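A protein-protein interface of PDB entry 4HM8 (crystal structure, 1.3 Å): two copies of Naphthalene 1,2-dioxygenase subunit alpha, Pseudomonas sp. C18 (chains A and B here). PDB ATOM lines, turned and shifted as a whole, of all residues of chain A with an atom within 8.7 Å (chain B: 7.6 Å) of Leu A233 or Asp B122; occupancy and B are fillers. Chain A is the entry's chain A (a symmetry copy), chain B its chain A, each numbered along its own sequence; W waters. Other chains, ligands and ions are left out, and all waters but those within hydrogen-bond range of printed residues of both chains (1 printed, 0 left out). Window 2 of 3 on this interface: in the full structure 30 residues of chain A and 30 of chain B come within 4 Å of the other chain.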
ATOM      1  N   ALA A 206      33.552  -5.964 -13.288  1.00  0.00           N
ATOM      2  CA  ALA A 206      33.055  -4.608 -13.056  1.00  0.00           C
ATOM      3  C   ALA A 206      33.614  -4.039 -11.757  1.00  0.00           C
ATOM      4  O   ALA A 206      33.704  -2.817 -11.596  1.00  0.00           O
ATOM      5  CB  ALA A 206      31.536  -4.578 -13.044  1.00  0.00           C
ATOM      6  N   TYR A 207      33.994  -4.927 -10.838  1.00  0.00           N
ATOM      7  CA  TYR A 207      34.480  -4.527  -9.510  1.00  0.00           C
ATOM      8  C   TYR A 207      35.676  -3.592  -9.633  1.00  0.00           C
ATOM      9  O   TYR A 207      35.806  -2.643  -8.859  1.00  0.00           O
ATOM     10  CB  TYR A 207      34.873  -5.776  -8.708  1.00  0.00           C
ATOM     11  CG  TYR A 207      35.007  -5.644  -7.194  1.00  0.00           C
ATOM     12  CD1 TYR A 207      34.574  -4.512  -6.504  1.00  0.00           C
ATOM     13  CD2 TYR A 207      35.553  -6.692  -6.451  1.00  0.00           C
ATOM     14  CE1 TYR A 207      34.693  -4.433  -5.109  1.00  0.00           C
ATOM     15  CE2 TYR A 207      35.668  -6.624  -5.078  1.00  0.00           C
ATOM     16  CZ  TYR A 207      35.237  -5.496  -4.414  1.00  0.00           C
ATOM     17  OH  TYR A 207      35.367  -5.455  -3.049  1.00  0.00           O
ATOM     18  N   GLY A 210      35.762   1.322 -10.787  1.00  0.00           N
ATOM     19  CA  GLY A 210      35.848   2.540  -9.992  1.00  0.00           C
ATOM     20  C   GLY A 210      37.224   2.799  -9.393  1.00  0.00           C
ATOM     21  O   GLY A 210      37.630   3.955  -9.224  1.00  0.00           O
ATOM     22  N   SER A 226      30.533   8.257 -12.216  1.00  0.00           N
ATOM     23  CA  SER A 226      30.173   8.346 -10.804  1.00  0.00           C
ATOM     24  C   SER A 226      30.922   7.320  -9.975  1.00  0.00           C
ATOM     25  O   SER A 226      30.869   7.332  -8.738  1.00  0.00           O
ATOM     26  CB  SER A 226      28.687   8.113 -10.624  1.00  0.00           C
ATOM     27  OG  SER A 226      28.317   6.814 -11.066  1.00  0.00           O
ATOM     28  N   LEU A 227      31.618   6.427 -10.663  1.00  0.00           N
ATOM     29  CA  LEU A 227      32.333   5.362 -10.004  1.00  0.00           C
ATOM     30  C   LEU A 227      33.730   5.778  -9.532  1.00  0.00           C
ATOM     31  O   LEU A 227      34.316   5.079  -8.731  1.00  0.00           O
ATOM     32  CB  LEU A 227      32.408   4.140 -10.929  1.00  0.00           C
ATOM     33  CG  LEU A 227      31.056   3.617 -11.427  1.00  0.00           C
ATOM     34  CD1 LEU A 227      31.226   2.420 -12.356  1.00  0.00           C
ATOM     35  CD2 LEU A 227      30.168   3.263 -10.256  1.00  0.00           C
ATOM     36  N   ALA A 228      34.259   6.910 -10.004  1.00  0.00           N
ATOM     37  CA  ALA A 228      35.677   7.249  -9.753  1.00  0.00           C
ATOM     38  C   ALA A 228      36.102   7.170  -8.283  1.00  0.00           C
ATOM     39  O   ALA A 228      35.496   7.805  -7.412  1.00  0.00           O
ATOM     40  CB  ALA A 228      36.039   8.619 -10.340  1.00  0.00           C
ATOM     41  N   GLY A 229      37.143   6.384  -8.014  1.00  0.00           N
ATOM     42  CA  GLY A 229      37.654   6.226  -6.662  1.00  0.00           C
ATOM     43  C   GLY A 229      36.681   5.528  -5.726  1.00  0.00           C
ATOM     44  O   GLY A 229      36.731   5.726  -4.510  1.00  0.00           O
ATOM     45  N   ASN A 230      35.801   4.701  -6.289  1.00  0.00           N
ATOM     46  CA  ASN A 230      34.739   4.056  -5.508  1.00  0.00           C
ATOM     47  C   ASN A 230      33.893   5.042  -4.710  1.00  0.00           C
ATOM     48  O   ASN A 230      33.474   4.761  -3.587  1.00  0.00           O
ATOM     49  CB  ASN A 230      35.295   2.943  -4.607  1.00  0.00           C
ATOM     50  CG  ASN A 230      35.673   1.712  -5.392  1.00  0.00           C
ATOM     51  OD1 ASN A 230      35.175   1.494  -6.501  1.00  0.00           O
ATOM     52  ND2 ASN A 230      36.548   0.891  -4.823  1.00  0.00           N
ATOM     53  N   ALA A 231      33.641   6.202  -5.305  1.00  0.00           N
ATOM     54  CA  ALA A 231      32.871   7.248  -4.655  1.00  0.00           C
ATOM     55  C   ALA A 231      31.411   6.837  -4.538  1.00  0.00           C
ATOM     56  O   ALA A 231      30.709   7.273  -3.637  1.00  0.00           O
ATOM     57  CB  ALA A 231      32.998   8.555  -5.425  1.00  0.00           C
ATOM     58  N   ALA A 232      30.956   5.999  -5.460  1.00  0.00           N
ATOM     59  CA  ALA A 232      29.578   5.546  -5.430  1.00  0.00           C
ATOM     60  C   ALA A 232      29.447   4.156  -6.029  1.00  0.00           C
ATOM     61  O   ALA A 232      30.188   3.783  -6.941  1.00  0.00           O
ATOM     62  CB  ALA A 232      28.680   6.530  -6.163  1.00  0.00           C
ATOM     63  N   LEU A 233      28.499   3.393  -5.503  1.00  0.00           N
ATOM     64  CA  LEU A 233      28.211   2.067  -6.016  1.00  0.00           C
ATOM     65  C   LEU A 233      27.057   2.182  -6.997  1.00  0.00           C
ATOM     66  O   LEU A 233      26.076   2.874  -6.709  1.00  0.00           O
ATOM     67  CB  LEU A 233      27.822   1.134  -4.867  1.00  0.00           C
ATOM     68  CG  LEU A 233      27.669  -0.353  -5.190  1.00  0.00           C
ATOM     69  CD1 LEU A 233      28.999  -0.956  -5.602  1.00  0.00           C
ATOM     70  CD2 LEU A 233      27.106  -1.101  -4.001  1.00  0.00           C
ATOM     71  N   PRO A 234      27.176   1.521  -8.161  1.00  0.00           N
ATOM     72  CA  PRO A 234      26.056   1.421  -9.098  1.00  0.00           C
ATOM     73  C   PRO A 234      24.860   0.903  -8.322  1.00  0.00           C
ATOM     74  O   PRO A 234      24.994  -0.088  -7.609  1.00  0.00           O
ATOM     75  CB  PRO A 234      26.534   0.365 -10.101  1.00  0.00           C
ATOM     76  CG  PRO A 234      28.016   0.428 -10.040  1.00  0.00           C
ATOM     77  CD  PRO A 234      28.347   0.752  -8.615  1.00  0.00           C
ATOM     78  N   PRO A 235      23.713   1.580  -8.440  1.00  0.00           N
ATOM     79  CA  PRO A 235      22.509   1.250  -7.673  1.00  0.00           C
ATOM     80  C   PRO A 235      22.015  -0.161  -7.955  1.00  0.00           C
ATOM     81  O   PRO A 235      22.411  -0.771  -8.949  1.00  0.00           O
ATOM     82  CB  PRO A 235      21.487   2.259  -8.196  1.00  0.00           C
ATOM     83  CG  PRO A 235      21.967   2.631  -9.544  1.00  0.00           C
ATOM     84  CD  PRO A 235      23.459   2.635  -9.434  1.00  0.00           C
ATOM     85  N   GLU A 236      21.154  -0.672  -7.082  1.00  0.00           N
ATOM     86  CA  GLU A 236      20.516  -1.963  -7.311  1.00  0.00           C
ATOM     87  C   GLU A 236      19.835  -1.967  -8.672  1.00  0.00           C
ATOM     88  O   GLU A 236      19.202  -0.983  -9.056  1.00  0.00           O
ATOM     89  CB  GLU A 236      19.486  -2.245  -6.210  1.00  0.00           C
ATOM     90  CG  GLU A 236      18.664  -3.517  -6.400  1.00  0.00           C
ATOM     91  CD  GLU A 236      19.457  -4.777  -6.099  1.00  0.00           C
ATOM     92  OE1 GLU A 236      20.615  -4.655  -5.638  1.00  0.00           O
ATOM     93  OE2 GLU A 236      18.923  -5.887  -6.325  1.00  0.00           O
ATOM     94  N   ALA A 238      21.292  -2.037 -11.558  1.00  0.00           N
ATOM     95  CA  ALA A 238      22.077  -1.314 -12.563  1.00  0.00           C
ATOM     96  C   ALA A 238      22.602  -2.235 -13.647  1.00  0.00           C
ATOM     97  O   ALA A 238      23.007  -1.778 -14.718  1.00  0.00           O
ATOM     98  CB  ALA A 238      23.228  -0.567 -11.915  1.00  0.00           C
ATOM     99  N   LEU A 253      25.684  -3.500 -18.286  1.00  0.00           N
ATOM    100  CA  LEU A 253      25.397  -2.297 -17.521  1.00  0.00           C
ATOM    101  C   LEU A 253      24.270  -1.573 -18.245  1.00  0.00           C
ATOM    102  O   LEU A 253      24.473  -1.003 -19.328  1.00  0.00           O
ATOM    103  CB  LEU A 253      26.644  -1.415 -17.400  1.00  0.00           C
ATOM    104  CG  LEU A 253      26.635  -0.343 -16.300  1.00  0.00           C
ATOM    105  CD1 LEU A 253      26.187  -0.921 -14.960  1.00  0.00           C
ATOM    106  CD2 LEU A 253      28.019   0.280 -16.154  1.00  0.00           C
ATOM    107  N   LEU A 387      32.937 -13.909  -5.488  1.00  0.00           N
ATOM    108  CA  LEU A 387      31.964 -12.834  -5.291  1.00  0.00           C
ATOM    109  C   LEU A 387      30.644 -13.177  -5.976  1.00  0.00           C
ATOM    110  O   LEU A 387      30.600 -13.430  -7.185  1.00  0.00           O
ATOM    111  CB  LEU A 387      32.516 -11.494  -5.794  1.00  0.00           C
ATOM    112  CG  LEU A 387      31.595 -10.278  -5.698  1.00  0.00           C
ATOM    113  CD1 LEU A 387      31.032 -10.139  -4.302  1.00  0.00           C
ATOM    114  CD2 LEU A 387      32.355  -9.023  -6.112  1.00  0.00           C
ATOM    115  N   GLY A 388      29.568 -13.212  -5.190  1.00  0.00           N
ATOM    116  CA  GLY A 388      28.252 -13.498  -5.730  1.00  0.00           C
ATOM    117  C   GLY A 388      27.919 -14.971  -5.801  1.00  0.00           C
ATOM    118  O   GLY A 388      26.808 -15.343  -6.196  1.00  0.00           O
ATOM    119  N   SER A 406      23.039  -8.835 -10.616  1.00  0.00           N
ATOM    120  CA  SER A 406      23.688  -7.694  -9.993  1.00  0.00           C
ATOM    121  C   SER A 406      24.783  -7.223 -10.936  1.00  0.00           C
ATOM    122  O   SER A 406      25.340  -8.027 -11.691  1.00  0.00           O
ATOM    123  CB  SER A 406      24.276  -8.073  -8.630  1.00  0.00           C
ATOM    124  OG  SER A 406      25.093  -9.228  -8.728  1.00  0.00           O
ATOM    125  N   ALA A 407      25.094  -5.932 -10.899  1.00  0.00           N
ATOM    126  CA  ALA A 407      26.048  -5.367 -11.848  1.00  0.00           C
ATOM    127  C   ALA A 407      27.488  -5.783 -11.576  1.00  0.00           C
ATOM    128  O   ALA A 407      28.284  -5.914 -12.508  1.00  0.00           O
ATOM    129  CB  ALA A 407      25.936  -3.858 -11.860  1.00  0.00           C
ATOM    130  N   ILE A 408      27.825  -5.985 -10.305  1.00  0.00           N
ATOM    131  CA  ILE A 408      29.195  -6.291  -9.907  1.00  0.00           C
ATOM    132  C   ILE A 408      29.297  -7.650  -9.232  1.00  0.00           C
ATOM    133  O   ILE A 408      28.676  -7.883  -8.194  1.00  0.00           O
ATOM    134  CB  ILE A 408      29.734  -5.236  -8.921  1.00  0.00           C
ATOM    135  CG1 ILE A 408      29.716  -3.842  -9.555  1.00  0.00           C
ATOM    136  CG2 ILE A 408      31.139  -5.612  -8.443  1.00  0.00           C
ATOM    137  CD1 ILE A 408      30.152  -2.743  -8.603  1.00  0.00           C
ATOM    138  N   PRO B 118      36.178  -2.926  -0.585  1.00  0.00           N
ATOM    139  CA  PRO B 118      35.211  -1.911  -1.025  1.00  0.00           C
ATOM    140  C   PRO B 118      33.810  -2.484  -1.174  1.00  0.00           C
ATOM    141  O   PRO B 118      33.646  -3.562  -1.758  1.00  0.00           O
ATOM    142  CB  PRO B 118      35.765  -1.459  -2.383  1.00  0.00           C
ATOM    143  CG  PRO B 118      37.241  -1.694  -2.261  1.00  0.00           C
ATOM    144  CD  PRO B 118      37.354  -2.983  -1.471  1.00  0.00           C
ATOM    145  N   PHE B 119      32.827  -1.782  -0.612  1.00  0.00           N
ATOM    146  CA  PHE B 119      31.420  -2.163  -0.695  1.00  0.00           C
ATOM    147  C   PHE B 119      31.170  -3.578  -0.191  1.00  0.00           C
ATOM    148  O   PHE B 119      30.326  -4.291  -0.736  1.00  0.00           O
ATOM    149  CB  PHE B 119      30.899  -2.008  -2.129  1.00  0.00           C
ATOM    150  CG  PHE B 119      31.178  -0.658  -2.730  1.00  0.00           C
ATOM    151  CD1 PHE B 119      30.606   0.489  -2.195  1.00  0.00           C
ATOM    152  CD2 PHE B 119      32.006  -0.538  -3.837  1.00  0.00           C
ATOM    153  CE1 PHE B 119      30.864   1.741  -2.753  1.00  0.00           C
ATOM    154  CE2 PHE B 119      32.266   0.704  -4.404  1.00  0.00           C
ATOM    155  CZ  PHE B 119      31.695   1.844  -3.862  1.00  0.00           C
ATOM    156  N   GLU B 120      31.890  -3.981   0.854  1.00  0.00           N
ATOM    157  CA  GLU B 120      31.816  -5.361   1.332  1.00  0.00           C
ATOM    158  C   GLU B 120      30.383  -5.771   1.641  1.00  0.00           C
ATOM    159  O   GLU B 120      29.926  -6.823   1.188  1.00  0.00           O
ATOM    160  CB  GLU B 120      32.716  -5.587   2.556  1.00  0.00           C
ATOM    161  CG  GLU B 120      32.728  -7.037   3.027  1.00  0.00           C
ATOM    162  CD  GLU B 120      33.545  -7.269   4.284  1.00  0.00           C
ATOM    163  OE1 GLU B 120      34.099  -6.299   4.849  1.00  0.00           O
ATOM    164  OE2 GLU B 120      33.624  -8.438   4.716  1.00  0.00           O
ATOM    165  N   LYS B 121      29.665  -4.918   2.365  1.00  0.00           N
ATOM    166  CA  LYS B 121      28.294  -5.214   2.762  1.00  0.00           C
ATOM    167  C   LYS B 121      27.380  -5.476   1.564  1.00  0.00           C
ATOM    168  O   LYS B 121      26.639  -6.461   1.542  1.00  0.00           O
ATOM    169  CB  LYS B 121      27.736  -4.064   3.609  1.00  0.00           C
ATOM    170  CG  LYS B 121      26.276  -4.221   4.001  1.00  0.00           C
ATOM    171  CD  LYS B 121      26.066  -5.452   4.860  1.00  0.00           C
ATOM    172  CE  LYS B 121      25.070  -5.176   5.976  1.00  0.00           C
ATOM    173  NZ  LYS B 121      25.569  -4.110   6.895  1.00  0.00           N
ATOM    174  N   ASP B 122      27.446  -4.605   0.562  1.00  0.00           N
ATOM    175  CA  ASP B 122      26.568  -4.731  -0.599  1.00  0.00           C
ATOM    176  C   ASP B 122      26.951  -5.880  -1.518  1.00  0.00           C
ATOM    177  O   ASP B 122      26.087  -6.454  -2.177  1.00  0.00           O
ATOM    178  CB  ASP B 122      26.533  -3.431  -1.404  1.00  0.00           C
ATOM    179  CG  ASP B 122      25.627  -2.382  -0.788  1.00  0.00           C
ATOM    180  OD1 ASP B 122      24.390  -2.552  -0.855  1.00  0.00           O
ATOM    181  OD2 ASP B 122      26.150  -1.384  -0.249  1.00  0.00           O
ATOM    182  N   LEU B 123      28.242  -6.203  -1.583  1.00  0.00           N
ATOM    183  CA  LEU B 123      28.725  -7.195  -2.542  1.00  0.00           C
ATOM    184  C   LEU B 123      28.854  -8.589  -1.939  1.00  0.00           C
ATOM    185  O   LEU B 123      28.302  -9.556  -2.468  1.00  0.00           O
ATOM    186  CB  LEU B 123      30.065  -6.752  -3.141  1.00  0.00           C
ATOM    187  CG  LEU B 123      30.022  -5.441  -3.935  1.00  0.00           C
ATOM    188  CD1 LEU B 123      31.404  -5.049  -4.437  1.00  0.00           C
ATOM    189  CD2 LEU B 123      29.052  -5.558  -5.101  1.00  0.00           C
ATOM    190  N   TYR B 124      29.586  -8.693  -0.834  1.00  0.00           N
ATOM    191  CA  TYR B 124      29.840  -9.987  -0.206  1.00  0.00           C
ATOM    192  C   TYR B 124      28.864 -10.307   0.914  1.00  0.00           C
ATOM    193  O   TYR B 124      28.732 -11.465   1.307  1.00  0.00           O
ATOM    194  CB  TYR B 124      31.259 -10.035   0.353  1.00  0.00           C
ATOM    195  CG  TYR B 124      32.336 -10.015  -0.702  1.00  0.00           C
ATOM    196  CD1 TYR B 124      32.769 -11.194  -1.292  1.00  0.00           C
ATOM    197  CD2 TYR B 124      32.924  -8.820  -1.104  1.00  0.00           C
ATOM    198  CE1 TYR B 124      33.760 -11.187  -2.251  1.00  0.00           C
ATOM    199  CE2 TYR B 124      33.911  -8.800  -2.064  1.00  0.00           C
ATOM    200  CZ  TYR B 124      34.329  -9.988  -2.631  1.00  0.00           C
ATOM    201  OH  TYR B 124      35.315  -9.969  -3.584  1.00  0.00           O
ATOM    202  N   GLY B 125      28.192  -9.286   1.436  1.00  0.00           N
ATOM    203  CA  GLY B 125      27.346  -9.474   2.600  1.00  0.00           C
ATOM    204  C   GLY B 125      28.209  -9.903   3.771  1.00  0.00           C
ATOM    205  O   GLY B 125      29.208  -9.252   4.080  1.00  0.00           O
ATOM    206  N   GLU B 126      27.834 -11.005   4.413  1.00  0.00           N
ATOM    207  CA  GLU B 126      28.613 -11.537   5.527  1.00  0.00           C
ATOM    208  C   GLU B 126      29.471 -12.730   5.098  1.00  0.00           C
ATOM    209  O   GLU B 126      30.055 -13.418   5.938  1.00  0.00           O
ATOM    210  CB  GLU B 126      27.669 -11.952   6.658  1.00  0.00           C
ATOM    211  CG  GLU B 126      26.759 -10.833   7.130  1.00  0.00           C
ATOM    212  CD  GLU B 126      27.517  -9.734   7.845  1.00  0.00           C
ATOM    213  OE1 GLU B 126      28.581 -10.036   8.423  1.00  0.00           O
ATOM    214  OE2 GLU B 126      27.054  -8.571   7.826  1.00  0.00           O
HETATM  215  O   HOH W   1      29.323 -12.839  -2.443  1.00  0.00           O
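Water W1 bridges the backbone NH (N) of Gly A388 (2.8 Å) and the backbone carbonyl oxygen (O) of Leu B123 (3.4 Å).
The backbone carbonyl oxygen of Pro B118 lies within hydrogen-bond range of the side-chain hydroxyl of Tyr A207, at 2.9 Å.
Leu B123 touches Tyr A207 (CD1 to CE1, 3.4 Å). CE2 of Tyr A207 touches OH of Tyr B124, 3.7 Å away. Asn A230 touches Pro B118 (ND2 to CB, 3.5 Å). Phe B119 touches Asn A230. Ala A232 touches Phe B119. Leu A233 touches Phe B119 (CD1 to CD2, 3.5 Å). Asp B122 touches Leu A233. O of Leu B123 touches CD1 of Leu A387, 3.3 Å away. CE1 of Tyr B124 touches CD1 of Leu A387, at 3.6 Å. CD2 of Leu B123 touches O of Ile A408 (3.9 Å).
Hydrophobic or aromatic side chains of chain A that line the printed part of chain B: Tyr A207, Leu A233, Leu A387 and Ile A408. Of the 9 printed residues of chain B, 5 touch a printed residue of chain A. Printed residues of chain B that touch a printed residue of chain A: Pro B118, Phe B119, Asp B122, Leu B123 and Tyr B124. Along chain B the printed residues that touch a printed residue of chain A span positions 118 to 124.
Leu A233 touches two residues of chain B. Asp B122 touches one residue of chain A. Of the printed residues of chain A, Leu B123 touches Tyr A207, Leu A387 and Ile A408. Printed residues of chain B within 4 Å of Ala A232: Phe B119 (3.9 Å). The nearest residue of chain A that does not touch Asp B122 is Glu A236 (6.4 Å). The nearest printed residue of chain B that does not touch Asn A230 is Leu B123 (7.8 Å).
No position is printed for both chains. Of the 11 pairs that touch across the chains among the printed residues, none has its exchanged pair printed and touching as well.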
